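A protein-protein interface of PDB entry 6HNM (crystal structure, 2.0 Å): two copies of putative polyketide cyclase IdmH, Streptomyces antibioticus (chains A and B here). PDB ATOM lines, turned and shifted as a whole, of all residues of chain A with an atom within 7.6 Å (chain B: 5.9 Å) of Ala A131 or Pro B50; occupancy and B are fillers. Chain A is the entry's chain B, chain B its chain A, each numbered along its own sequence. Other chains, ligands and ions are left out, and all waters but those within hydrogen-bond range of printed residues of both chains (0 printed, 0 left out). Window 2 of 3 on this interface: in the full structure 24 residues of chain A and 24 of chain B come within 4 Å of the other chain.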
ATOM      1  N   ASP A 125      26.704 -23.995  14.296  1.00  0.00           N
ATOM      2  CA  ASP A 125      27.267 -22.733  14.759  1.00  0.00           C
ATOM      3  C   ASP A 125      27.739 -22.834  16.231  1.00  0.00           C
ATOM      4  O   ASP A 125      27.193 -22.170  17.125  1.00  0.00           O
ATOM      5  CB  ASP A 125      26.227 -21.628  14.581  1.00  0.00           C
ATOM      6  CG  ASP A 125      26.808 -20.236  14.768  1.00  0.00           C
ATOM      7  OD1 ASP A 125      28.037 -20.087  14.918  1.00  0.00           O
ATOM      8  OD2 ASP A 125      26.023 -19.269  14.765  1.00  0.00           O
ATOM      9  N   ASN A 126      28.766 -23.647  16.456  1.00  0.00           N
ATOM     10  CA  ASN A 126      29.286 -23.935  17.807  1.00  0.00           C
ATOM     11  C   ASN A 126      29.782 -22.705  18.569  1.00  0.00           C
ATOM     12  O   ASN A 126      29.572 -22.604  19.779  1.00  0.00           O
ATOM     13  CB  ASN A 126      30.409 -24.981  17.759  1.00  0.00           C
ATOM     14  CG  ASN A 126      29.931 -26.324  17.205  1.00  0.00           C
ATOM     15  OD1 ASN A 126      30.540 -26.884  16.293  1.00  0.00           O
ATOM     16  ND2 ASN A 126      28.841 -26.843  17.757  1.00  0.00           N
ATOM     17  N   VAL A 127      30.422 -21.771  17.870  1.00  0.00           N
ATOM     18  CA  VAL A 127      30.973 -20.575  18.524  1.00  0.00           C
ATOM     19  C   VAL A 127      29.862 -19.708  19.145  1.00  0.00           C
ATOM     20  O   VAL A 127      30.029 -19.192  20.252  1.00  0.00           O
ATOM     21  CB  VAL A 127      31.883 -19.759  17.579  1.00  0.00           C
ATOM     22  CG1 VAL A 127      32.395 -18.490  18.268  1.00  0.00           C
ATOM     23  CG2 VAL A 127      33.062 -20.624  17.126  1.00  0.00           C
ATOM     24  N   THR A 128      28.729 -19.580  18.456  1.00  0.00           N
ATOM     25  CA  THR A 128      27.553 -18.885  19.012  1.00  0.00           C
ATOM     26  C   THR A 128      26.998 -19.601  20.253  1.00  0.00           C
ATOM     27  O   THR A 128      26.650 -18.944  21.247  1.00  0.00           O
ATOM     28  CB  THR A 128      26.442 -18.713  17.955  1.00  0.00           C
ATOM     29  OG1 THR A 128      26.916 -17.832  16.933  1.00  0.00           O
ATOM     30  CG2 THR A 128      25.134 -18.133  18.554  1.00  0.00           C
ATOM     31  N   MET A 129      26.916 -20.929  20.197  1.00  0.00           N
ATOM     32  CA  MET A 129      26.468 -21.733  21.352  1.00  0.00           C
ATOM     33  C   MET A 129      27.359 -21.552  22.579  1.00  0.00           C
ATOM     34  O   MET A 129      26.857 -21.442  23.695  1.00  0.00           O
ATOM     35  CB  MET A 129      26.410 -23.220  21.003  1.00  0.00           C
ATOM     36  CG  MET A 129      25.998 -24.108  22.172  1.00  0.00           C
ATOM     37  SD  MET A 129      26.040 -25.848  21.740  1.00  0.00           S
ATOM     38  CE  MET A 129      27.819 -26.123  21.727  1.00  0.00           C
ATOM     39  N   LEU A 130      28.670 -21.560  22.356  1.00  0.00           N
ATOM     40  CA  LEU A 130      29.639 -21.377  23.433  1.00  0.00           C
ATOM     41  C   LEU A 130      29.600 -19.941  23.988  1.00  0.00           C
ATOM     42  O   LEU A 130      29.814 -19.740  25.184  1.00  0.00           O
ATOM     43  CB  LEU A 130      31.056 -21.747  22.971  1.00  0.00           C
ATOM     44  CG  LEU A 130      31.278 -23.195  22.511  1.00  0.00           C
ATOM     45  CD1 LEU A 130      32.695 -23.356  21.978  1.00  0.00           C
ATOM     46  CD2 LEU A 130      30.991 -24.203  23.611  1.00  0.00           C
ATOM     47  N   ALA A 131      29.308 -18.958  23.134  1.00  0.00           N
ATOM     48  CA  ALA A 131      29.127 -17.581  23.589  1.00  0.00           C
ATOM     49  C   ALA A 131      27.950 -17.467  24.567  1.00  0.00           C
ATOM     50  O   ALA A 131      28.059 -16.782  25.591  1.00  0.00           O
ATOM     51  CB  ALA A 131      28.937 -16.644  22.405  1.00  0.00           C
ATOM     52  N   GLN A 132      26.847 -18.157  24.255  1.00  0.00           N
ATOM     53  CA  GLN A 132      25.644 -18.171  25.104  1.00  0.00           C
ATOM     54  C   GLN A 132      25.857 -18.843  26.472  1.00  0.00           C
ATOM     55  O   GLN A 132      25.289 -18.400  27.466  1.00  0.00           O
ATOM     56  CB  GLN A 132      24.476 -18.857  24.382  1.00  0.00           C
ATOM     57  CG  GLN A 132      23.944 -18.095  23.179  1.00  0.00           C
ATOM     58  CD  GLN A 132      23.089 -18.955  22.250  1.00  0.00           C
ATOM     59  OE1 GLN A 132      22.935 -20.169  22.446  1.00  0.00           O
ATOM     60  NE2 GLN A 132      22.529 -18.321  21.220  1.00  0.00           N
ATOM     61  N   LEU A 133      26.649 -19.912  26.505  1.00  0.00           N
ATOM     62  CA  LEU A 133      26.973 -20.608  27.753  1.00  0.00           C
ATOM     63  C   LEU A 133      28.116 -19.907  28.496  1.00  0.00           C
ATOM     64  O   LEU A 133      27.958 -19.510  29.653  1.00  0.00           O
ATOM     65  CB  LEU A 133      27.361 -22.066  27.481  1.00  0.00           C
ATOM     66  CG  LEU A 133      26.313 -22.926  26.761  1.00  0.00           C
ATOM     67  CD1 LEU A 133      26.892 -24.303  26.473  1.00  0.00           C
ATOM     68  CD2 LEU A 133      24.980 -22.975  27.503  1.00  0.00           C
ATOM     69  N   GLY A 134      29.269 -19.788  27.842  1.00  0.00           N
ATOM     70  CA  GLY A 134      30.488 -19.250  28.459  1.00  0.00           C
ATOM     71  C   GLY A 134      31.391 -20.363  28.957  1.00  0.00           C
ATOM     72  O   GLY A 134      31.530 -21.401  28.307  1.00  0.00           O
ATOM     73  N   PRO B  40      27.962 -16.742  11.360  1.00  0.00           N
ATOM     74  CA  PRO B  40      28.301 -17.604  12.484  1.00  0.00           C
ATOM     75  C   PRO B  40      29.071 -16.878  13.583  1.00  0.00           C
ATOM     76  O   PRO B  40      29.613 -15.788  13.350  1.00  0.00           O
ATOM     77  CB  PRO B  40      29.146 -18.697  11.840  1.00  0.00           C
ATOM     78  CG  PRO B  40      29.767 -18.046  10.649  1.00  0.00           C
ATOM     79  CD  PRO B  40      28.865 -16.933  10.208  1.00  0.00           C
ATOM     80  N   GLY B  41      29.132 -17.500  14.760  1.00  0.00           N
ATOM     81  CA  GLY B  41      29.752 -16.911  15.954  1.00  0.00           C
ATOM     82  C   GLY B  41      31.208 -16.508  15.779  1.00  0.00           C
ATOM     83  O   GLY B  41      31.650 -15.554  16.425  1.00  0.00           O
ATOM     84  N   THR B  42      31.934 -17.204  14.890  1.00  0.00           N
ATOM     85  CA  THR B  42      33.308 -16.827  14.532  1.00  0.00           C
ATOM     86  C   THR B  42      33.403 -15.386  13.994  1.00  0.00           C
ATOM     87  O   THR B  42      34.407 -14.709  14.219  1.00  0.00           O
ATOM     88  CB  THR B  42      33.940 -17.793  13.491  1.00  0.00           C
ATOM     89  OG1 THR B  42      33.155 -17.826  12.292  1.00  0.00           O
ATOM     90  CG2 THR B  42      34.074 -19.220  14.036  1.00  0.00           C
ATOM     91  N   GLY B  44      31.469 -12.940  15.008  1.00  0.00           N
ATOM     92  CA  GLY B  44      31.158 -12.016  16.091  1.00  0.00           C
ATOM     93  C   GLY B  44      32.401 -11.282  16.560  1.00  0.00           C
ATOM     94  O   GLY B  44      33.525 -11.784  16.431  1.00  0.00           O
ATOM     95  N   ASP B  45      32.200 -10.085  17.100  1.00  0.00           N
ATOM     96  CA  ASP B  45      33.299  -9.333  17.737  1.00  0.00           C
ATOM     97  C   ASP B  45      32.808  -8.519  18.935  1.00  0.00           C
ATOM     98  O   ASP B  45      31.677  -8.731  19.406  1.00  0.00           O
ATOM     99  CB  ASP B  45      34.074  -8.501  16.689  1.00  0.00           C
ATOM    100  CG  ASP B  45      33.366  -7.226  16.286  1.00  0.00           C
ATOM    101  OD1 ASP B  45      32.136  -7.098  16.450  1.00  0.00           O
ATOM    102  OD2 ASP B  45      34.057  -6.327  15.783  1.00  0.00           O
ATOM    103  N   HIS B  48      29.654  -6.490  17.824  1.00  0.00           N
ATOM    104  CA  HIS B  48      28.546  -7.341  17.341  1.00  0.00           C
ATOM    105  C   HIS B  48      28.667  -8.753  17.933  1.00  0.00           C
ATOM    106  O   HIS B  48      29.410  -9.575  17.389  1.00  0.00           O
ATOM    107  CB  HIS B  48      28.538  -7.415  15.811  1.00  0.00           C
ATOM    108  CG  HIS B  48      28.274  -6.104  15.138  1.00  0.00           C
ATOM    109  ND1 HIS B  48      29.268  -5.183  14.877  1.00  0.00           N
ATOM    110  CD2 HIS B  48      27.124  -5.554  14.684  1.00  0.00           C
ATOM    111  CE1 HIS B  48      28.744  -4.135  14.269  1.00  0.00           C
ATOM    112  NE2 HIS B  48      27.443  -4.330  14.149  1.00  0.00           N
ATOM    113  N   PRO B  49      27.962  -9.023  19.052  1.00  0.00           N
ATOM    114  CA  PRO B  49      28.136 -10.326  19.707  1.00  0.00           C
ATOM    115  C   PRO B  49      27.592 -11.477  18.857  1.00  0.00           C
ATOM    116  O   PRO B  49      26.601 -11.276  18.156  1.00  0.00           O
ATOM    117  CB  PRO B  49      27.345 -10.197  21.022  1.00  0.00           C
ATOM    118  CG  PRO B  49      26.460  -9.016  20.848  1.00  0.00           C
ATOM    119  CD  PRO B  49      27.084  -8.122  19.823  1.00  0.00           C
ATOM    120  N   PRO B  50      28.227 -12.671  18.928  1.00  0.00           N
ATOM    121  CA  PRO B  50      27.739 -13.892  18.266  1.00  0.00           C
ATOM    122  C   PRO B  50      26.227 -14.098  18.380  1.00  0.00           C
ATOM    123  O   PRO B  50      25.660 -13.942  19.465  1.00  0.00           O
ATOM    124  CB  PRO B  50      28.477 -15.006  19.018  1.00  0.00           C
ATOM    125  CG  PRO B  50      29.772 -14.385  19.415  1.00  0.00           C
ATOM    126  CD  PRO B  50      29.497 -12.921  19.650  1.00  0.00           C
ATOM    127  N   GLY B  51      25.581 -14.414  17.257  1.00  0.00           N
ATOM    128  CA  GLY B  51      24.128 -14.560  17.208  1.00  0.00           C
ATOM    129  C   GLY B  51      23.366 -13.318  16.775  1.00  0.00           C
ATOM    130  O   GLY B  51      22.216 -13.429  16.362  1.00  0.00           O
ATOM    131  N   THR B  52      23.991 -12.141  16.860  1.00  0.00           N
ATOM    132  CA  THR B  52      23.370 -10.884  16.426  1.00  0.00           C
ATOM    133  C   THR B  52      23.398 -10.801  14.896  1.00  0.00           C
ATOM    134  O   THR B  52      24.476 -10.841  14.318  1.00  0.00           O
ATOM    135  CB  THR B  52      24.137  -9.654  16.982  1.00  0.00           C
ATOM    136  OG1 THR B  52      24.328  -9.802  18.388  1.00  0.00           O
ATOM    137  CG2 THR B  52      23.382  -8.367  16.707  1.00  0.00           C
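Asp A125 touches Pro B40. Gly B41 touches Val A127 (C to CG1, 3.4 Å). CG2 of Thr B42 touches CG2 of Val A127, at 3.5 Å. Pro B50 touches Thr A128 (CB to OG1, 3.8 Å). Thr A128 touches Gly B51. Ala A131 touches Pro B50.
The side-chain carboxylate (OD2) of Asp A125 is in hydrogen-bond range of the side-chain hydroxyl (OG1) of Thr A128, at 2.8 Å.
The backbone NH (N) of Gly B41 sits at hydrogen-bond distance from the side-chain hydroxyl (OG1) of Thr A128. N of Gly B41 lies within hydrogen-bond range of OD1 of Asp A125 (2.8 Å).
No position is printed for both chains.
Hydrophobic or aromatic side chains of chain B that line the printed part of chain A: Pro B40 and Pro B50. Among the printed residues, 8 pairs touch across the chains.
Leu A133 touches none of the printed residues of chain B. Of the printed residues of chain A, Pro B40 touches Asp A125. Pro B50 touches just these residues of chain A: Thr A128 (3.8 Å) and Ala A131 (3.8 Å). Printed residues of chain A within 4 Å of Gly B51: Thr A128. The nearest printed residue of chain B that does not touch Ala A131 is Pro B49 (6.4 Å). The nearest residue of chain A that does not touch Pro B50 is Val A127 (4.6 Å). The nearest printed residue of chain B that does not touch Asp A125 is Thr B42 (4.8 Å).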
